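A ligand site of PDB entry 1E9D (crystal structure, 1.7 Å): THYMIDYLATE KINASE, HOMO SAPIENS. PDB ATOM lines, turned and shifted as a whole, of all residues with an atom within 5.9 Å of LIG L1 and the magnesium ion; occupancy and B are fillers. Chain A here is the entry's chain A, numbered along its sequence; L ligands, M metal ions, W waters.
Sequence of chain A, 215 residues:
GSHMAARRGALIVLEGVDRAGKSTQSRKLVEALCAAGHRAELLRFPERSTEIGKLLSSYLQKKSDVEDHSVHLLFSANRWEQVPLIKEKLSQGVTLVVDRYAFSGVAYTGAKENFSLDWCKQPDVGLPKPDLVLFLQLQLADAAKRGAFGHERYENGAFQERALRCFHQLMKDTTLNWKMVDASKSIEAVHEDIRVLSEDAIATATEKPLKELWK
The backbone NH of Ser 23 sits close to an oxygen (O2) of LIG L1 (3.0 Å). The backbone NH (N) of Thr 24 is in hydrogen-bond range of an oxygen (O5) of LIG L1, at 2.8 Å. An oxygen (O5) of LIG L1 lies within hydrogen-bond range of the side-chain hydroxyl (OG1) of Thr 24, 2.6 Å away. The backbone NH (N) of Lys 22 lies within hydrogen-bond range of an oxygen (O1) of LIG L1, 2.9 Å away. The side-chain amino group (NZ) of Lys 22 is in salt-bridge range of an oxygen (O1) of LIG L1 (2.7 Å). The backbone carbonyl oxygen of Lys 185 is in hydrogen-bond range of a nitrogen (N3) of LIG L1 (2.9 Å). The backbone NH (N) of Gly 21 sits at hydrogen-bond distance from an oxygen (O1) of LIG L1 (3.0 Å). An oxygen (O3) of LIG L1 lies within hydrogen-bond range of the backbone NH (N) of Arg 19, 3.1 Å away. An oxygen (O1) of LIG L1 is in hydrogen-bond range of the backbone NH (N) of Ala 20, at 3.2 Å. The guanidinium group (NH2) of Arg 146 sits close to a nitrogen (N4) of LIG L1 (3.4 Å). The guanidinium group (NE) of Arg 100 lies within salt-bridge range of an oxygen (O2) of LG2 L2, 2.8 Å away.
OG of Ser 23 sits close to OD2 of Asp 99. The side-chain hydroxyl (OG1) of Thr 24 lies close to the guanidinium group (NH2) of Arg 27 (3.5 Å). O of Val 17 is in hydrogen-bond range of NZ of Lys 22, 2.8 Å away. NH1 of Arg 146 lies within hydrogen-bond range of O of Arg 19 (3.1 Å). The guanidinium group (NE) of Arg 19 is in salt-bridge range of the side-chain carboxylate (OD2) of Asp 18 (3.4 Å). The backbone carbonyl oxygen of Ala 20 is in hydrogen-bond range of the guanidinium group of Arg 146 (3.4 Å). The side-chain amide nitrogen (NE2) of Gln 25 is in hydrogen-bond range of the backbone carbonyl oxygen (O) of Ile 187, at 3.0 Å. O of Ala 183 sits at hydrogen-bond distance from NH2 of Arg 146 (2.8 Å).
A nitrogen (N3) of LIG L1 lies close to the backbone NH of Ile 187, 3.5 Å away. Merely in contact with LIG L1: Ser 186 (3.7 Å), Val 17 (3.9 Å) and Ala 183 (3.9 Å). Hydrophobic or aromatic side chains that line LIG L1: Ile 187. 12 residues have an atom within 4 Å of LIG L1: Val 17, Arg 19, Ala 20, Gly 21, Lys 22, Ser 23, Thr 24, Arg 146, Ala 183, Lys 185, Ser 186 and Ile 187.
One residue has an atom within 4 Å of the magnesium ion: Ser 23. The nearest printed residue that does not touch the magnesium ion is Asp 99 (4.1 Å).
The magnesium ion is bound by an oxygen (O2) of LIG L1 (2.0 Å), water W3 (2.1 Å), the side-chain hydroxyl of Ser 23 (2.1 Å), water W16 (2.2 Å), water W9 (2.2 Å) and water W15 (2.2 Å).
Water W16 bridges an oxygen (O2) of LG2 L2 and the side-chain carboxylate (OD1) of Asp 99. Water W4 bridges an oxygen (O10) of LIG L1 (2.5 Å) and the side-chain hydroxyl (OG1) of Thr 24 (2.7 Å). Water W13 lies within hydrogen-bond range of N2 of LIG L1 (2.7 Å) and NE2 of Gln 25 (2.7 Å). Water W7 lies within hydrogen-bond range of the guanidinium group (NH2) of Arg 100, an oxygen (O3) of LIG L1, an oxygen (O1) of LG2 L2, the side-chain amino group (NZ) of Lys 22 and the side-chain carboxylate (OD1) of Asp 18. Water W6 lies within hydrogen-bond range of an oxygen (O4) of LIG L1 (3.0 Å) and the guanidinium group of Arg 27 (3.1 Å). Water W14 lies within hydrogen-bond range of the backbone carbonyl oxygen (O) of Ala 20 (2.7 Å), the backbone carbonyl oxygen (O) of Ala 183 (2.7 Å), the guanidinium group (NH1) of Arg 146 (3.1 Å) and a nitrogen (N3) of LIG L1 (3.2 Å).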
ATOM      1  N   GLY A  16      11.166 -20.935  16.584  1.00  0.00           N
ATOM      2  CA  GLY A  16      12.600 -21.157  16.384  1.00  0.00           C
ATOM      3  C   GLY A  16      13.315 -19.809  16.256  1.00  0.00           C
ATOM      4  O   GLY A  16      12.666 -18.793  16.087  1.00  0.00           O
ATOM      5  N   VAL A  17      14.649 -19.834  16.261  1.00  0.00           N
ATOM      6  CA  VAL A  17      15.373 -18.577  16.131  1.00  0.00           C
ATOM      7  C   VAL A  17      15.266 -18.018  14.720  1.00  0.00           C
ATOM      8  O   VAL A  17      14.749 -18.631  13.813  1.00  0.00           O
ATOM      9  CB  VAL A  17      16.884 -18.714  16.399  1.00  0.00           C
ATOM     10  CG1 VAL A  17      17.155 -18.935  17.869  1.00  0.00           C
ATOM     11  CG2 VAL A  17      17.443 -19.824  15.505  1.00  0.00           C
ATOM     12  N   ASP A  18      15.864 -16.835  14.565  1.00  0.00           N
ATOM     13  CA  ASP A  18      15.951 -16.163  13.283  1.00  0.00           C
ATOM     14  C   ASP A  18      16.660 -17.034  12.236  1.00  0.00           C
ATOM     15  O   ASP A  18      17.648 -17.685  12.555  1.00  0.00           O
ATOM     16  CB  ASP A  18      16.801 -14.904  13.558  1.00  0.00           C
ATOM     17  CG  ASP A  18      16.651 -13.942  12.409  1.00  0.00           C
ATOM     18  OD1 ASP A  18      15.501 -13.498  12.171  1.00  0.00           O
ATOM     19  OD2 ASP A  18      17.721 -13.712  11.795  1.00  0.00           O
ATOM     20  N   ARG A  19      16.092 -17.143  11.055  1.00  0.00           N
ATOM     21  CA  ARG A  19      16.643 -17.917   9.939  1.00  0.00           C
ATOM     22  C   ARG A  19      16.582 -19.422  10.084  1.00  0.00           C
ATOM     23  O   ARG A  19      17.173 -20.158   9.284  1.00  0.00           O
ATOM     24  CB  ARG A  19      18.089 -17.437   9.707  1.00  0.00           C
ATOM     25  CG  ARG A  19      18.003 -15.943   9.308  1.00  0.00           C
ATOM     26  CD  ARG A  19      19.376 -15.447   8.915  1.00  0.00           C
ATOM     27  NE  ARG A  19      20.205 -15.162  10.069  1.00  0.00           N
ATOM     28  CZ  ARG A  19      21.524 -15.001   9.943  1.00  0.00           C
ATOM     29  NH1 ARG A  19      22.090 -15.130   8.739  1.00  0.00           N
ATOM     30  NH2 ARG A  19      22.251 -14.729  11.008  1.00  0.00           N
ATOM     31  N   ALA A  20      15.765 -19.895  11.010  1.00  0.00           N
ATOM     32  CA  ALA A  20      15.598 -21.302  11.281  1.00  0.00           C
ATOM     33  C   ALA A  20      14.817 -21.960  10.169  1.00  0.00           C
ATOM     34  O   ALA A  20      14.912 -23.187  10.072  1.00  0.00           O
ATOM     35  CB  ALA A  20      14.921 -21.436  12.642  1.00  0.00           C
ATOM     36  N   GLY A  21      14.096 -21.188   9.344  1.00  0.00           N
ATOM     37  CA  GLY A  21      13.294 -21.710   8.252  1.00  0.00           C
ATOM     38  C   GLY A  21      11.786 -21.668   8.490  1.00  0.00           C
ATOM     39  O   GLY A  21      11.044 -22.398   7.852  1.00  0.00           O
ATOM     40  N   LYS A  22      11.347 -20.943   9.535  1.00  0.00           N
ATOM     41  CA  LYS A  22       9.940 -20.955   9.891  1.00  0.00           C
ATOM     42  C   LYS A  22       8.988 -20.514   8.784  1.00  0.00           C
ATOM     43  O   LYS A  22       7.959 -21.108   8.514  1.00  0.00           O
ATOM     44  CB  LYS A  22       9.705 -19.994  11.090  1.00  0.00           C
ATOM     45  CG  LYS A  22      10.498 -20.434  12.325  1.00  0.00           C
ATOM     46  CD  LYS A  22      10.338 -19.475  13.488  1.00  0.00           C
ATOM     47  CE  LYS A  22      10.764 -18.034  13.259  1.00  0.00           C
ATOM     48  NZ  LYS A  22      12.189 -17.868  12.851  1.00  0.00           N
ATOM     49  N   SER A  23       9.330 -19.405   8.137  1.00  0.00           N
ATOM     50  CA  SER A  23       8.440 -18.916   7.052  1.00  0.00           C
ATOM     51  C   SER A  23       8.477 -19.890   5.847  1.00  0.00           C
ATOM     52  O   SER A  23       7.373 -20.147   5.328  1.00  0.00           O
ATOM     53  CB  SER A  23       8.881 -17.517   6.670  1.00  0.00           C
ATOM     54  OG  SER A  23       8.705 -16.650   7.806  1.00  0.00           O
ATOM     55  N   THR A  24       9.656 -20.297   5.466  1.00  0.00           N
ATOM     56  CA  THR A  24       9.708 -21.264   4.329  1.00  0.00           C
ATOM     57  C   THR A  24       8.896 -22.499   4.713  1.00  0.00           C
ATOM     58  O   THR A  24       8.148 -22.987   3.914  1.00  0.00           O
ATOM     59  CB  THR A  24      11.154 -21.653   4.032  1.00  0.00           C
ATOM     60  OG1 THR A  24      11.892 -20.464   3.711  1.00  0.00           O
ATOM     61  CG2 THR A  24      11.332 -22.653   2.880  1.00  0.00           C
ATOM     62  N   GLN A  25       9.157 -23.136   5.872  1.00  0.00           N
ATOM     63  CA  GLN A  25       8.426 -24.356   6.195  1.00  0.00           C
ATOM     64  C   GLN A  25       6.945 -24.093   6.442  1.00  0.00           C
ATOM     65  O   GLN A  25       6.180 -24.989   6.127  1.00  0.00           O
ATOM     66  CB  GLN A  25       9.073 -25.050   7.409  1.00  0.00           C
ATOM     67  CG  GLN A  25      10.526 -25.444   7.151  1.00  0.00           C
ATOM     68  CD  GLN A  25      10.687 -26.441   6.013  1.00  0.00           C
ATOM     69  OE1 GLN A  25       9.750 -27.140   5.704  1.00  0.00           O
ATOM     70  NE2 GLN A  25      11.853 -26.550   5.355  1.00  0.00           N
ATOM     71  N   ARG A  27       4.928 -22.052   4.863  1.00  0.00           N
ATOM     72  CA  ARG A  27       4.350 -21.968   3.528  1.00  0.00           C
ATOM     73  C   ARG A  27       4.274 -23.362   2.901  1.00  0.00           C
ATOM     74  O   ARG A  27       3.245 -23.669   2.278  1.00  0.00           O
ATOM     75  CB  ARG A  27       5.204 -21.073   2.597  1.00  0.00           C
ATOM     76  CG  ARG A  27       5.109 -19.581   2.942  1.00  0.00           C
ATOM     77  CD  ARG A  27       5.766 -18.734   1.833  1.00  0.00           C
ATOM     78  NE  ARG A  27       7.181 -19.020   1.675  1.00  0.00           N
ATOM     79  CZ  ARG A  27       8.217 -18.432   2.274  1.00  0.00           C
ATOM     80  NH1 ARG A  27       8.007 -17.419   3.122  1.00  0.00           N
ATOM     81  NH2 ARG A  27       9.427 -18.842   1.897  1.00  0.00           N
ATOM     82  N   ASP A  99       3.145 -19.063  11.802  1.00  0.00           N
ATOM     83  CA  ASP A  99       4.588 -18.773  11.809  1.00  0.00           C
ATOM     84  C   ASP A  99       4.873 -17.810  12.986  1.00  0.00           C
ATOM     85  O   ASP A  99       4.545 -16.612  12.870  1.00  0.00           O
ATOM     86  CB  ASP A  99       4.788 -18.060  10.456  1.00  0.00           C
ATOM     87  CG  ASP A  99       6.195 -17.616  10.155  1.00  0.00           C
ATOM     88  OD1 ASP A  99       7.114 -17.741  11.027  1.00  0.00           O
ATOM     89  OD2 ASP A  99       6.404 -17.137   9.022  1.00  0.00           O
ATOM     90  N   ARG A 100       5.239 -18.379  14.114  1.00  0.00           N
ATOM     91  CA  ARG A 100       5.468 -17.693  15.376  1.00  0.00           C
ATOM     92  C   ARG A 100       4.134 -17.483  16.153  1.00  0.00           C
ATOM     93  O   ARG A 100       3.054 -17.281  15.597  1.00  0.00           O
ATOM     94  CB  ARG A 100       6.178 -16.360  15.282  1.00  0.00           C
ATOM     95  CG  ARG A 100       7.633 -16.342  14.853  1.00  0.00           C
ATOM     96  CD  ARG A 100       8.171 -14.884  15.051  1.00  0.00           C
ATOM     97  NE  ARG A 100       9.503 -14.748  14.513  1.00  0.00           N
ATOM     98  CZ  ARG A 100      10.667 -15.121  14.977  1.00  0.00           C
ATOM     99  NH1 ARG A 100      10.841 -15.774  16.116  1.00  0.00           N
ATOM    100  NH2 ARG A 100      11.729 -14.818  14.232  1.00  0.00           N
ATOM    101  N   ARG A 146      23.199 -18.833   6.691  1.00  0.00           N
ATOM    102  CA  ARG A 146      22.091 -18.576   5.773  1.00  0.00           C
ATOM    103  C   ARG A 146      22.095 -17.095   5.417  1.00  0.00           C
ATOM    104  O   ARG A 146      21.148 -16.417   5.777  1.00  0.00           O
ATOM    105  CB  ARG A 146      20.734 -18.998   6.350  1.00  0.00           C
ATOM    106  CG  ARG A 146      20.665 -20.522   6.417  1.00  0.00           C
ATOM    107  CD  ARG A 146      19.563 -21.062   7.342  1.00  0.00           C
ATOM    108  NE  ARG A 146      19.773 -22.513   7.379  1.00  0.00           N
ATOM    109  CZ  ARG A 146      18.890 -23.415   7.782  1.00  0.00           C
ATOM    110  NH1 ARG A 146      17.728 -22.971   8.226  1.00  0.00           N
ATOM    111  NH2 ARG A 146      19.209 -24.702   7.755  1.00  0.00           N
ATOM    112  N   ALA A 183      16.356 -28.476  11.976  1.00  0.00           N
ATOM    113  CA  ALA A 183      16.258 -27.495  10.916  1.00  0.00           C
ATOM    114  C   ALA A 183      17.543 -27.308  10.125  1.00  0.00           C
ATOM    115  O   ALA A 183      17.617 -26.472   9.229  1.00  0.00           O
ATOM    116  CB  ALA A 183      15.782 -26.174  11.551  1.00  0.00           C
ATOM    117  N   SER A 184      18.570 -28.083  10.449  1.00  0.00           N
ATOM    118  CA  SER A 184      19.860 -27.973   9.768  1.00  0.00           C
ATOM    119  C   SER A 184      19.846 -28.726   8.446  1.00  0.00           C
ATOM    120  O   SER A 184      20.725 -28.581   7.605  1.00  0.00           O
ATOM    121  CB  SER A 184      20.985 -28.497  10.671  1.00  0.00           C
ATOM    122  OG  SER A 184      20.968 -29.922  10.684  1.00  0.00           O
ATOM    123  N   LYS A 185      18.820 -29.580   8.287  1.00  0.00           N
ATOM    124  CA  LYS A 185      18.768 -30.369   7.049  1.00  0.00           C
ATOM    125  C   LYS A 185      18.354 -29.499   5.866  1.00  0.00           C
ATOM    126  O   LYS A 185      18.240 -28.292   6.032  1.00  0.00           O
ATOM    127  CB  LYS A 185      17.894 -31.610   7.190  1.00  0.00           C
ATOM    128  CG  LYS A 185      18.379 -32.547   8.302  1.00  0.00           C
ATOM    129  CD  LYS A 185      17.198 -33.130   9.075  1.00  0.00           C
ATOM    130  CE  LYS A 185      16.858 -34.552   8.674  1.00  0.00           C
ATOM    131  NZ  LYS A 185      15.703 -35.131   9.420  1.00  0.00           N
ATOM    132  N   SER A 186      18.104 -30.136   4.727  1.00  0.00           N
ATOM    133  CA  SER A 186      17.682 -29.461   3.517  1.00  0.00           C
ATOM    134  C   SER A 186      16.223 -29.010   3.665  1.00  0.00           C
ATOM    135  O   SER A 186      15.512 -29.546   4.493  1.00  0.00           O
ATOM    136  CB  SER A 186      17.724 -30.405   2.317  1.00  0.00           C
ATOM    137  OG  SER A 186      16.727 -31.438   2.347  1.00  0.00           O
ATOM    138  N   ILE A 187      15.850 -28.022   2.862  1.00  0.00           N
ATOM    139  CA  ILE A 187      14.460 -27.544   2.879  1.00  0.00           C
ATOM    140  C   ILE A 187      13.488 -28.714   2.662  1.00  0.00           C
ATOM    141  O   ILE A 187      12.546 -28.807   3.470  1.00  0.00           O
ATOM    142  CB  ILE A 187      14.285 -26.409   1.860  1.00  0.00           C
ATOM    143  CG1 ILE A 187      15.022 -25.154   2.336  1.00  0.00           C
ATOM    144  CG2 ILE A 187      12.799 -26.154   1.594  1.00  0.00           C
ATOM    145  CD1 ILE A 187      14.946 -23.980   1.373  1.00  0.00           C
ATOM    146  N   VAL A 190      13.620 -31.180   5.884  1.00  0.00           N
ATOM    147  CA  VAL A 190      12.952 -30.592   7.037  1.00  0.00           C
ATOM    148  C   VAL A 190      11.442 -30.616   6.860  1.00  0.00           C
ATOM    149  O   VAL A 190      10.643 -30.988   7.719  1.00  0.00           O
ATOM    150  CB  VAL A 190      13.467 -29.153   7.232  1.00  0.00           C
ATOM    151  CG1 VAL A 190      12.717 -28.449   8.370  1.00  0.00           C
ATOM    152  CG2 VAL A 190      14.961 -29.198   7.565  1.00  0.00           C
HETATM  153  P1  LIG L   1      12.653 -17.636   9.289  1.00  0.00           P
HETATM  154  O1  LIG L   1      12.921 -18.637  10.385  1.00  0.00           O
HETATM  155  O2  LIG L   1      11.313 -17.281   8.876  1.00  0.00           O
HETATM  156  O3  LIG L   1      13.512 -16.323   9.525  1.00  0.00           O
HETATM  157  P2  LIG L   1      13.187 -18.324   6.466  1.00  0.00           P
HETATM  158  O4  LIG L   1      12.883 -16.975   5.987  1.00  0.00           O
HETATM  159  O5  LIG L   1      12.260 -19.439   6.088  1.00  0.00           O
HETATM  160  O6  LIG L   1      13.483 -18.342   8.041  1.00  0.00           O
HETATM  161  O7  LIG L   1      14.620 -18.734   5.926  1.00  0.00           O
HETATM  162  C1  LIG L   1      15.797 -17.914   6.086  1.00  0.00           C
HETATM  163  C2  LIG L   1      16.715 -18.049   4.846  1.00  0.00           C
HETATM  164  O8  LIG L   1      17.284 -19.348   4.889  1.00  0.00           O
HETATM  165  C3  LIG L   1      15.959 -17.864   3.540  1.00  0.00           C
HETATM  166  O9  LIG L   1      16.802 -17.311   2.547  1.00  0.00           O
HETATM  167  C4  LIG L   1      15.685 -19.355   3.194  1.00  0.00           C
HETATM  168  O10 LIG L   1      15.637 -19.643   1.846  1.00  0.00           O
HETATM  169  C5  LIG L   1      16.913 -20.056   3.754  1.00  0.00           C
HETATM  170  N1  LIG L   1      16.588 -21.437   4.191  1.00  0.00           N
HETATM  171  C6  LIG L   1      15.414 -21.841   4.797  1.00  0.00           C
HETATM  172  N2  LIG L   1      15.430 -23.108   5.176  1.00  0.00           N
HETATM  173  C7  LIG L   1      16.716 -23.556   4.786  1.00  0.00           C
HETATM  174  C8  LIG L   1      17.349 -24.799   4.912  1.00  0.00           C
HETATM  175  N3  LIG L   1      16.743 -25.831   5.433  1.00  0.00           N
HETATM  176  N4  LIG L   1      18.600 -24.804   4.408  1.00  0.00           N
HETATM  177  C9  LIG L   1      19.228 -23.755   3.880  1.00  0.00           C
HETATM  178  N5  LIG L   1      18.675 -22.553   3.721  1.00  0.00           N
HETATM  179  C10 LIG L   1      17.461 -22.554   4.207  1.00  0.00           C
HETATM  180  P1  LG2 L   2       9.634 -12.556  11.913  1.00  0.00           P
HETATM  181  O1  LG2 L   2      11.090 -12.861  12.016  1.00  0.00           O
HETATM  182  O2  LG2 L   2       8.754 -13.759  11.958  1.00  0.00           O
HETATM  183  O3  LG2 L   2       9.349 -11.542  10.830  1.00  0.00           O
HETATM  184  O4  LG2 L   2       9.232 -11.769  13.294  1.00  0.00           O
HETATM  185  C1  LG2 L   2       9.808 -10.450  13.458  1.00  0.00           C
HETATM  186  C2  LG2 L   2      10.267 -10.221  14.937  1.00  0.00           C
HETATM  187  O5  LG2 L   2       9.259 -10.152  15.927  1.00  0.00           O
HETATM  188  C3  LG2 L   2      11.248 -11.285  15.346  1.00  0.00           C
HETATM  189  N1  LG2 L   2      12.552 -10.633  15.765  1.00  0.00           N
HETATM  190  N2  LG2 L   2      13.498 -11.413  15.851  1.00  0.00           N
HETATM  191  N3  LG2 L   2      14.342 -12.165  15.925  1.00  0.00           N
HETATM  192  C4  LG2 L   2      10.589 -11.986  16.563  1.00  0.00           C
HETATM  193  C5  LG2 L   2       9.644 -10.852  17.076  1.00  0.00           C
HETATM  194  N4  LG2 L   2       8.528 -11.145  17.945  1.00  0.00           N
HETATM  195  C6  LG2 L   2       8.488 -10.552  19.247  1.00  0.00           C
HETATM  196  O6  LG2 L   2       9.437  -9.888  19.681  1.00  0.00           O
HETATM  197  N5  LG2 L   2       7.312 -10.806  19.908  1.00  0.00           N
HETATM  198  C7  LG2 L   2       6.247 -11.532  19.393  1.00  0.00           C
HETATM  199  O7  LG2 L   2       5.091 -11.753  20.087  1.00  0.00           O
HETATM  200  C8  LG2 L   2       6.352 -12.131  18.016  1.00  0.00           C
HETATM  201  C9  LG2 L   2       5.254 -12.914  17.422  1.00  0.00           C
HETATM  202  C10 LG2 L   2       7.517 -11.832  17.372  1.00  0.00           C
HETATM  203 MG    MG M   1      10.237 -15.650   8.784  1.00  0.00          MG
HETATM  204  O   HOH W   1      20.587 -26.702   5.513  1.00  0.00           O
HETATM  205  O   HOH W   2      18.524 -24.296   0.666  1.00  0.00           O
HETATM  206  O   HOH W   3      11.184 -15.244   6.991  1.00  0.00           O
HETATM  207  O   HOH W   4      13.179 -19.678   1.417  1.00  0.00           O
HETATM  208  O   HOH W   5      20.484 -20.531   2.603  1.00  0.00           O
HETATM  209  O   HOH W   6      11.248 -16.969   3.525  1.00  0.00           O
HETATM  210  O   HOH W   7      12.718 -15.197  11.891  1.00  0.00           O
HETATM  211  O   HOH W   8      17.477 -21.466   0.244  1.00  0.00           O
HETATM  212  O   HOH W   9       8.903 -13.883   8.558  1.00  0.00           O
HETATM  213  O   HOH W  10      14.884 -14.656   8.039  1.00  0.00           O
HETATM  214  O   HOH W  11      20.174 -17.746   2.930  1.00  0.00           O
HETATM  215  O   HOH W  12      16.234 -14.599   3.300  1.00  0.00           O
HETATM  216  O   HOH W  13      13.991 -25.141   6.151  1.00  0.00           O
HETATM  217  O   HOH W  14      15.465 -25.098   8.261  1.00  0.00           O
HETATM  218  O   HOH W  15      11.652 -14.309   9.893  1.00  0.00           O
HETATM  219  O   HOH W  16       9.100 -16.013  10.624  1.00  0.00           O
